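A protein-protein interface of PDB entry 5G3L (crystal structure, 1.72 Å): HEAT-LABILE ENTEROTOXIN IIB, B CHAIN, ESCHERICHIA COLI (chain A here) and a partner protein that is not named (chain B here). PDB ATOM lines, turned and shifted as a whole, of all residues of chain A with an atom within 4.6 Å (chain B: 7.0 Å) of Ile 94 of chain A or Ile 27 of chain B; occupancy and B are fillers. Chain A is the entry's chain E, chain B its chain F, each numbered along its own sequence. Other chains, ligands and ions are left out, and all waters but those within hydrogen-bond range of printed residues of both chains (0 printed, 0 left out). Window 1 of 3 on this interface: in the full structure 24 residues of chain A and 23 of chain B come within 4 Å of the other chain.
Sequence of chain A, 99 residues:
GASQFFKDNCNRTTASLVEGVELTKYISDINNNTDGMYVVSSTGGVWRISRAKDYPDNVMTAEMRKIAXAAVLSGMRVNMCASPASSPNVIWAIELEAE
Among the printed residues, pairs that only touch across the chains: Phe 5 of chain A with Ile 27 of chain B (3.7 Å), Phe 5 of chain A with Tyr 38 of chain B (3.6 Å), Phe 5 of chain A with Val 46 of chain B (3.9 Å), Phe 6 of chain A with Ile 27 of chain B (3.9 Å), Met 64 of chain A with Ser 28 of chain B (3.6 Å), Ile 67 of chain A with Tyr 26 of chain B (3.7 Å), Ala 93 of chain A with Ser 28 of chain B (3.3 Å), Ala 93 of chain A with Asp 29 of chain B (3.9 Å), Ile 94 of chain A with Tyr 26 of chain B (3.8 Å), Ile 94 of chain A with Ile 27 of chain B (3.4 Å), Glu 95 of chain A with Lys 25 of chain B (3.5 Å), Glu 95 of chain A with Tyr 26 of chain B (3.3 Å), Glu 95 of chain A with Ile 27 of chain B (3.3 Å) and Leu 96 of chain A with Lys 25 of chain B (3.1 Å).
Printed residues of chain B within 4 Å of Ile 94 of chain A: Tyr 26 (3.8 Å), Ile 27 (3.4 Å) and Ser 28 (3.0 Å). Ile 27 of chain B touches just these residues of chain A: Phe 5 (3.7 Å), Phe 6 (3.9 Å), Ile 94 (3.4 Å) and Glu 95 (3.3 Å). Printed residues of chain B within 4 Å of Met 64 of chain A: Ser 28 (3.6 Å). Printed residues of chain A within 4 Å of Ser 28 of chain B: Met 64 (3.6 Å), Ala 93 (3.3 Å) and Ile 94 (3.0 Å). Of the printed residues of chain A, Val 46 of chain B touches Phe 5. Of the printed residues of chain A, Tyr 26 of chain B touches Ile 67 (3.7 Å), Ile 94 (3.8 Å), Glu 95 (3.3 Å) and Leu 96 (2.8 Å). Printed residues of chain B within 4 Å of Phe 6 of chain A: Ile 27 (3.9 Å). The nearest residue of chain A that does not touch Ile 27 of chain B is Ser 3 of chain A (4.05 Å).
O of Ser 28 of chain B sits at hydrogen-bond distance from N of Ile 94 of chain A (3.0 Å). O of Tyr 26 of chain B is in hydrogen-bond range of N of Leu 96 of chain A (2.8 Å).
OG of Ser 3 of chain A sits at hydrogen-bond distance from N of Phe 6 of chain A (3.1 Å). O of Asn 79 of chain A lies within hydrogen-bond range of N of Glu 95 of chain A, 2.9 Å away. The backbone carbonyl oxygen of Lys 25 of chain B sits at hydrogen-bond distance from the backbone NH of Val 40 of chain B. The backbone carbonyl oxygen (O) of Tyr 38 of chain B lies within hydrogen-bond range of the backbone NH (N) of Ile 27 of chain B (2.9 Å). The side-chain hydroxyl (OG) of Ser 28 of chain B lies within hydrogen-bond range of the side-chain sulfur (SD) of Met 37 of chain B (3.6 Å). The backbone NH (N) of Gly 36 of chain B sits at hydrogen-bond distance from the backbone carbonyl oxygen (O) of Asp 29 of chain B, at 2.9 Å.
Of the 14 printed residues of chain B, 7 touch a printed residue of chain A. Along chain A the printed residues that touch a printed residue of chain B span positions 5 to 96. Among the printed residues, no Asp or Glu carboxylate lies within 4 Å of a Lys or Arg side-chain nitrogen of the other chain.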
ATOM      1  N   SER A   3      18.265 -28.533  16.323  1.00  0.00           N
ATOM      2  CA  SER A   3      19.662 -28.554  15.797  1.00  0.00           C
ATOM      3  C   SER A   3      20.042 -30.013  15.461  1.00  0.00           C
ATOM      4  O   SER A   3      19.591 -30.972  16.079  1.00  0.00           O
ATOM      5  CB  SER A   3      20.660 -27.939  16.794  1.00  0.00           C
ATOM      6  OG  SER A   3      20.744 -28.725  17.959  1.00  0.00           O
ATOM      7  N   PHE A   5      22.821 -31.354  16.148  1.00  0.00           N
ATOM      8  CA  PHE A   5      23.445 -31.806  17.345  1.00  0.00           C
ATOM      9  C   PHE A   5      22.435 -32.405  18.356  1.00  0.00           C
ATOM     10  O   PHE A   5      22.641 -33.496  18.861  1.00  0.00           O
ATOM     11  CB  PHE A   5      24.211 -30.605  17.971  1.00  0.00           C
ATOM     12  CG  PHE A   5      24.875 -30.888  19.276  1.00  0.00           C
ATOM     13  CD1 PHE A   5      26.029 -31.609  19.334  1.00  0.00           C
ATOM     14  CD2 PHE A   5      24.351 -30.317  20.467  1.00  0.00           C
ATOM     15  CE1 PHE A   5      26.667 -31.838  20.560  1.00  0.00           C
ATOM     16  CE2 PHE A   5      25.004 -30.533  21.676  1.00  0.00           C
ATOM     17  CZ  PHE A   5      26.129 -31.288  21.729  1.00  0.00           C
ATOM     18  N   PHE A   6      21.358 -31.664  18.610  1.00  0.00           N
ATOM     19  CA  PHE A   6      20.307 -32.133  19.503  1.00  0.00           C
ATOM     20  C   PHE A   6      19.669 -33.447  19.001  1.00  0.00           C
ATOM     21  O   PHE A   6      19.483 -34.376  19.758  1.00  0.00           O
ATOM     22  CB  PHE A   6      19.251 -31.044  19.707  1.00  0.00           C
ATOM     23  CG  PHE A   6      18.254 -31.372  20.817  1.00  0.00           C
ATOM     24  CD1 PHE A   6      18.541 -31.073  22.133  1.00  0.00           C
ATOM     25  CD2 PHE A   6      17.034 -31.967  20.522  1.00  0.00           C
ATOM     26  CE1 PHE A   6      17.603 -31.327  23.119  1.00  0.00           C
ATOM     27  CE2 PHE A   6      16.096 -32.182  21.501  1.00  0.00           C
ATOM     28  CZ  PHE A   6      16.378 -31.895  22.800  1.00  0.00           C
ATOM     29  N   MET A  64      16.702 -27.080  32.892  1.00  0.00           N
ATOM     30  CA  MET A  64      15.448 -27.500  32.232  1.00  0.00           C
ATOM     31  C   MET A  64      14.241 -26.716  32.746  1.00  0.00           C
ATOM     32  O   MET A  64      13.365 -26.318  31.999  1.00  0.00           O
ATOM     33  CB  MET A  64      15.157 -29.019  32.462  1.00  0.00           C
ATOM     34  CG  MET A  64      16.192 -29.863  31.825  1.00  0.00           C
ATOM     35  SD  MET A  64      15.725 -31.616  32.048  1.00  0.00           S
ATOM     36  CE  MET A  64      16.901 -32.457  31.037  1.00  0.00           C
ATOM     37  N   ILE A  67      14.393 -23.192  31.313  1.00  0.00           N
ATOM     38  CA  ILE A  67      13.970 -23.247  29.895  1.00  0.00           C
ATOM     39  C   ILE A  67      12.410 -23.332  29.802  1.00  0.00           C
ATOM     40  O   ILE A  67      11.752 -22.619  29.036  1.00  0.00           O
ATOM     41  CB  ILE A  67      14.666 -24.413  29.183  1.00  0.00           C
ATOM     42  CG1 ILE A  67      16.136 -24.064  28.905  1.00  0.00           C
ATOM     43  CG2 ILE A  67      13.908 -24.781  27.922  1.00  0.00           C
ATOM     44  CD1 ILE A  67      16.986 -25.212  28.490  1.00  0.00           C
ATOM     45  N   VAL A  78      10.167 -25.196  22.006  1.00  0.00           N
ATOM     46  CA  VAL A  78      11.180 -26.131  22.472  1.00  0.00           C
ATOM     47  C   VAL A  78      11.191 -27.421  21.636  1.00  0.00           C
ATOM     48  O   VAL A  78      10.157 -27.841  21.057  1.00  0.00           O
ATOM     49  CB  VAL A  78      11.035 -26.505  23.956  1.00  0.00           C
ATOM     50  CG1 VAL A  78      11.076 -25.248  24.832  1.00  0.00           C
ATOM     51  CG2 VAL A  78       9.715 -27.246  24.203  1.00  0.00           C
ATOM     52  N   ASN A  79      12.338 -28.070  21.640  1.00  0.00           N
ATOM     53  CA  ASN A  79      12.476 -29.402  21.194  1.00  0.00           C
ATOM     54  C   ASN A  79      12.828 -30.281  22.358  1.00  0.00           C
ATOM     55  O   ASN A  79      13.642 -29.905  23.189  1.00  0.00           O
ATOM     56  CB  ASN A  79      13.543 -29.497  20.108  1.00  0.00           C
ATOM     57  CG  ASN A  79      13.357 -28.451  19.028  1.00  0.00           C
ATOM     58  OD1 ASN A  79      12.314 -28.369  18.384  1.00  0.00           O
ATOM     59  ND2 ASN A  79      14.379 -27.561  18.855  1.00  0.00           N
ATOM     60  N   MET A  80      12.214 -31.447  22.456  1.00  0.00           N
ATOM     61  CA  MET A  80      12.415 -32.349  23.577  1.00  0.00           C
ATOM     62  C   MET A  80      12.913 -33.728  23.166  1.00  0.00           C
ATOM     63  O   MET A  80      12.541 -34.233  22.096  1.00  0.00           O
ATOM     64  CB  MET A  80      11.142 -32.488  24.415  1.00  0.00           C
ATOM     65  CG  MET A  80      10.810 -31.194  25.155  1.00  0.00           C
ATOM     66  SD  MET A  80       9.274 -31.161  26.077  1.00  0.00           S
ATOM     67  CE  MET A  80       8.114 -31.359  24.762  1.00  0.00           C
ATOM     68  N   ILE A  91      11.320 -35.803  30.371  1.00  0.00           N
ATOM     69  CA  ILE A  91      12.306 -35.030  29.568  1.00  0.00           C
ATOM     70  C   ILE A  91      13.739 -35.291  29.982  1.00  0.00           C
ATOM     71  O   ILE A  91      14.164 -35.054  31.118  1.00  0.00           O
ATOM     72  CB  ILE A  91      12.014 -33.535  29.644  1.00  0.00           C
ATOM     73  CG1 ILE A  91      10.651 -33.202  29.084  1.00  0.00           C
ATOM     74  CG2 ILE A  91      13.073 -32.765  28.889  1.00  0.00           C
ATOM     75  CD1 ILE A  91      10.122 -31.834  29.547  1.00  0.00           C
ATOM     76  N   ALA A  93      16.354 -34.427  27.690  1.00  0.00           N
ATOM     77  CA  ALA A  93      17.014 -33.233  27.091  1.00  0.00           C
ATOM     78  C   ALA A  93      16.009 -32.285  26.501  1.00  0.00           C
ATOM     79  O   ALA A  93      14.927 -32.707  26.009  1.00  0.00           O
ATOM     80  CB  ALA A  93      18.031 -33.639  26.016  1.00  0.00           C
ATOM     81  N   ILE A  94      16.332 -30.993  26.535  1.00  0.00           N
ATOM     82  CA  ILE A  94      15.441 -29.973  26.007  1.00  0.00           C
ATOM     83  C   ILE A  94      16.268 -28.868  25.368  1.00  0.00           C
ATOM     84  O   ILE A  94      17.374 -28.544  25.860  1.00  0.00           O
ATOM     85  CB  ILE A  94      14.441 -29.439  27.085  1.00  0.00           C
ATOM     86  CG1 ILE A  94      13.404 -28.546  26.500  1.00  0.00           C
ATOM     87  CG2 ILE A  94      15.229 -28.810  28.219  1.00  0.00           C
ATOM     88  CD1 ILE A  94      12.209 -28.289  27.430  1.00  0.00           C
ATOM     89  N   GLU A  95      15.740 -28.311  24.280  1.00  0.00           N
ATOM     90  CA  GLU A  95      16.377 -27.282  23.507  1.00  0.00           C
ATOM     91  C   GLU A  95      15.389 -26.113  23.333  1.00  0.00           C
ATOM     92  O   GLU A  95      14.335 -26.275  22.751  1.00  0.00           O
ATOM     93  CB  GLU A  95      16.802 -27.811  22.125  1.00  0.00           C
ATOM     94  CG  GLU A  95      17.447 -26.770  21.185  1.00  0.00           C
ATOM     95  CD  GLU A  95      18.024 -27.463  19.950  1.00  0.00           C
ATOM     96  OE1 GLU A  95      17.200 -27.938  19.107  1.00  0.00           O
ATOM     97  OE2 GLU A  95      19.247 -27.475  19.751  1.00  0.00           O
ATOM     98  N   LEU A  96      15.745 -24.961  23.899  1.00  0.00           N
ATOM     99  CA  LEU A  96      14.974 -23.742  23.711  1.00  0.00           C
ATOM    100  C   LEU A  96      15.426 -23.050  22.417  1.00  0.00           C
ATOM    101  O   LEU A  96      16.641 -22.903  22.218  1.00  0.00           O
ATOM    102  CB  LEU A  96      15.245 -22.792  24.894  1.00  0.00           C
ATOM    103  CG  LEU A  96      14.559 -21.435  24.875  1.00  0.00           C
ATOM    104  CD1 LEU A  96      13.047 -21.597  25.032  1.00  0.00           C
ATOM    105  CD2 LEU A  96      15.060 -20.575  26.036  1.00  0.00           C
ATOM    106  N   LYS B  25      19.804 -21.122  20.068  1.00  0.00           N
ATOM    107  CA  LYS B  25      19.366 -22.301  20.817  1.00  0.00           C
ATOM    108  C   LYS B  25      20.160 -22.477  22.102  1.00  0.00           C
ATOM    109  O   LYS B  25      21.365 -22.295  22.130  1.00  0.00           O
ATOM    110  CB  LYS B  25      19.410 -23.552  19.976  1.00  0.00           C
ATOM    111  CG  LYS B  25      18.701 -23.363  18.611  1.00  0.00           C
ATOM    112  CD  LYS B  25      18.396 -24.656  17.918  1.00  0.00           C
ATOM    113  CE  LYS B  25      18.070 -24.494  16.436  1.00  0.00           C
ATOM    114  NZ  LYS B  25      16.710 -23.996  16.195  1.00  0.00           N
ATOM    115  N   TYR B  26      19.477 -22.952  23.123  1.00  0.00           N
ATOM    116  CA  TYR B  26      20.111 -23.347  24.407  1.00  0.00           C
ATOM    117  C   TYR B  26      19.621 -24.750  24.826  1.00  0.00           C
ATOM    118  O   TYR B  26      18.420 -25.013  24.839  1.00  0.00           O
ATOM    119  CB  TYR B  26      19.692 -22.336  25.439  1.00  0.00           C
ATOM    120  CG  TYR B  26      20.249 -22.487  26.836  1.00  0.00           C
ATOM    121  CD1 TYR B  26      21.585 -22.596  27.066  1.00  0.00           C
ATOM    122  CD2 TYR B  26      19.395 -22.467  27.944  1.00  0.00           C
ATOM    123  CE1 TYR B  26      22.079 -22.632  28.354  1.00  0.00           C
ATOM    124  CE2 TYR B  26      19.886 -22.506  29.217  1.00  0.00           C
ATOM    125  CZ  TYR B  26      21.237 -22.562  29.402  1.00  0.00           C
ATOM    126  OH  TYR B  26      21.787 -22.587  30.686  1.00  0.00           O
ATOM    127  N   ILE B  27      20.573 -25.617  25.159  1.00  0.00           N
ATOM    128  CA  ILE B  27      20.361 -27.040  25.421  1.00  0.00           C
ATOM    129  C   ILE B  27      20.786 -27.470  26.826  1.00  0.00           C
ATOM    130  O   ILE B  27      21.908 -27.188  27.212  1.00  0.00           O
ATOM    131  CB  ILE B  27      21.118 -27.929  24.389  1.00  0.00           C
ATOM    132  CG1 ILE B  27      20.706 -27.649  22.933  1.00  0.00           C
ATOM    133  CG2 ILE B  27      20.910 -29.408  24.756  1.00  0.00           C
ATOM    134  CD1 ILE B  27      21.626 -28.255  21.882  1.00  0.00           C
ATOM    135  N   SER B  28      19.873 -28.183  27.511  1.00  0.00           N
ATOM    136  CA  SER B  28      20.167 -28.893  28.718  1.00  0.00           C
ATOM    137  C   SER B  28      19.922 -30.366  28.515  1.00  0.00           C
ATOM    138  O   SER B  28      18.867 -30.736  28.059  1.00  0.00           O
ATOM    139  CB  SER B  28      19.328 -28.398  29.909  1.00  0.00           C
ATOM    140  OG  SER B  28      19.690 -29.213  31.068  1.00  0.00           O
ATOM    141  N   ASP B  29      20.946 -31.177  28.768  1.00  0.00           N
ATOM    142  CA  ASP B  29      20.916 -32.626  28.447  1.00  0.00           C
ATOM    143  C   ASP B  29      21.459 -33.450  29.637  1.00  0.00           C
ATOM    144  O   ASP B  29      22.541 -33.111  30.152  1.00  0.00           O
ATOM    145  CB  ASP B  29      21.776 -32.798  27.174  1.00  0.00           C
ATOM    146  CG  ASP B  29      21.798 -34.214  26.620  1.00  0.00           C
ATOM    147  OD1 ASP B  29      21.699 -35.177  27.385  1.00  0.00           O
ATOM    148  OD2 ASP B  29      22.044 -34.344  25.389  1.00  0.00           O
ATOM    149  N   ILE B  30      20.714 -34.477  30.109  1.00  0.00           N
ATOM    150  CA  ILE B  30      21.242 -35.320  31.196  1.00  0.00           C
ATOM    151  C   ILE B  30      21.603 -36.739  30.723  1.00  0.00           C
ATOM    152  O   ILE B  30      21.804 -37.615  31.544  1.00  0.00           O
ATOM    153  CB  ILE B  30      20.381 -35.376  32.460  1.00  0.00           C
ATOM    154  CG1 ILE B  30      18.964 -35.875  32.168  1.00  0.00           C
ATOM    155  CG2 ILE B  30      20.406 -33.993  33.118  1.00  0.00           C
ATOM    156  CD1 ILE B  30      18.249 -36.264  33.459  1.00  0.00           C
ATOM    157  N   THR B  34      26.397 -37.433  26.656  1.00  0.00           N
ATOM    158  CA  THR B  34      26.144 -36.096  26.092  1.00  0.00           C
ATOM    159  C   THR B  34      25.720 -35.063  27.130  1.00  0.00           C
ATOM    160  O   THR B  34      25.327 -33.960  26.783  1.00  0.00           O
ATOM    161  CB  THR B  34      25.076 -36.134  24.961  1.00  0.00           C
ATOM    162  OG1 THR B  34      23.827 -36.660  25.461  1.00  0.00           O
ATOM    163  CG2 THR B  34      25.586 -36.998  23.821  1.00  0.00           C
ATOM    164  N   GLY B  36      25.243 -32.236  29.666  1.00  0.00           N
ATOM    165  CA  GLY B  36      25.861 -30.926  29.741  1.00  0.00           C
ATOM    166  C   GLY B  36      24.954 -29.836  29.267  1.00  0.00           C
ATOM    167  O   GLY B  36      23.764 -30.099  28.931  1.00  0.00           O
ATOM    168  N   MET B  37      25.524 -28.621  29.227  1.00  0.00           N
ATOM    169  CA  MET B  37      24.831 -27.424  28.741  1.00  0.00           C
ATOM    170  C   MET B  37      25.524 -26.909  27.485  1.00  0.00           C
ATOM    171  O   MET B  37      26.775 -26.829  27.432  1.00  0.00           O
ATOM    172  CB  MET B  37      24.854 -26.303  29.812  1.00  0.00           C
ATOM    173  CG  MET B  37      24.218 -26.719  31.173  1.00  0.00           C
ATOM    174  SD  MET B  37      22.502 -27.035  30.979  1.00  0.00           S
ATOM    175  CE  MET B  37      21.905 -25.634  30.074  1.00  0.00           C
ATOM    176  N   TYR B  38      24.746 -26.632  26.446  1.00  0.00           N
ATOM    177  CA  TYR B  38      25.266 -26.222  25.130  1.00  0.00           C
ATOM    178  C   TYR B  38      24.494 -25.041  24.535  1.00  0.00           C
ATOM    179  O   TYR B  38      23.309 -24.799  24.848  1.00  0.00           O
ATOM    180  CB  TYR B  38      25.247 -27.359  24.120  1.00  0.00           C
ATOM    181  CG  TYR B  38      25.881 -28.615  24.630  1.00  0.00           C
ATOM    182  CD1 TYR B  38      25.112 -29.542  25.309  1.00  0.00           C
ATOM    183  CD2 TYR B  38      27.202 -28.941  24.339  1.00  0.00           C
ATOM    184  CE1 TYR B  38      25.657 -30.737  25.737  1.00  0.00           C
ATOM    185  CE2 TYR B  38      27.750 -30.128  24.779  1.00  0.00           C
ATOM    186  CZ  TYR B  38      26.976 -31.023  25.490  1.00  0.00           C
ATOM    187  OH  TYR B  38      27.475 -32.272  25.910  1.00  0.00           O
ATOM    188  N   VAL B  39      25.194 -24.269  23.722  1.00  0.00           N
ATOM    189  CA  VAL B  39      24.537 -23.233  22.917  1.00  0.00           C
ATOM    190  C   VAL B  39      24.819 -23.471  21.410  1.00  0.00           C
ATOM    191  O   VAL B  39      25.824 -24.052  21.041  1.00  0.00           O
ATOM    192  CB  VAL B  39      24.997 -21.828  23.288  1.00  0.00           C
ATOM    193  CG1 VAL B  39      24.600 -21.461  24.720  1.00  0.00           C
ATOM    194  CG2 VAL B  39      26.507 -21.657  23.116  1.00  0.00           C
ATOM    195  N   VAL B  40      23.866 -23.036  20.589  1.00  0.00           N
ATOM    196  CA  VAL B  40      23.935 -23.164  19.132  1.00  0.00           C
ATOM    197  C   VAL B  40      23.742 -21.777  18.547  1.00  0.00           C
ATOM    198  O   VAL B  40      22.810 -21.041  18.925  1.00  0.00           O
ATOM    199  CB  VAL B  40      22.851 -24.114  18.563  1.00  0.00           C
ATOM    200  CG1 VAL B  40      23.127 -24.361  17.097  1.00  0.00           C
ATOM    201  CG2 VAL B  40      22.820 -25.449  19.339  1.00  0.00           C
ATOM    202  N   VAL B  46      28.209 -24.944  17.442  1.00  0.00           N
ATOM    203  CA  VAL B  46      27.838 -25.495  18.778  1.00  0.00           C
ATOM    204  C   VAL B  46      29.001 -25.318  19.737  1.00  0.00           C
ATOM    205  O   VAL B  46      30.161 -25.648  19.400  1.00  0.00           O
ATOM    206  CB  VAL B  46      27.505 -26.971  18.680  1.00  0.00           C
ATOM    207  CG1 VAL B  46      27.056 -27.529  20.035  1.00  0.00           C
ATOM    208  CG2 VAL B  46      26.442 -27.212  17.606  1.00  0.00           C
ATOM    209  N   ILE B  49      29.220 -25.206  27.509  1.00  0.00           N
ATOM    210  CA  ILE B  49      29.473 -24.372  28.705  1.00  0.00           C
ATOM    211  C   ILE B  49      30.052 -25.302  29.773  1.00  0.00           C
ATOM    212  O   ILE B  49      29.470 -26.304  30.025  1.00  0.00           O
ATOM    213  CB  ILE B  49      28.163 -23.732  29.229  1.00  0.00           C
ATOM    214  CG1 ILE B  49      27.441 -22.993  28.110  1.00  0.00           C
ATOM    215  CG2 ILE B  49      28.461 -22.859  30.410  1.00  0.00           C
ATOM    216  CD1 ILE B  49      26.047 -22.440  28.464  1.00  0.00           C
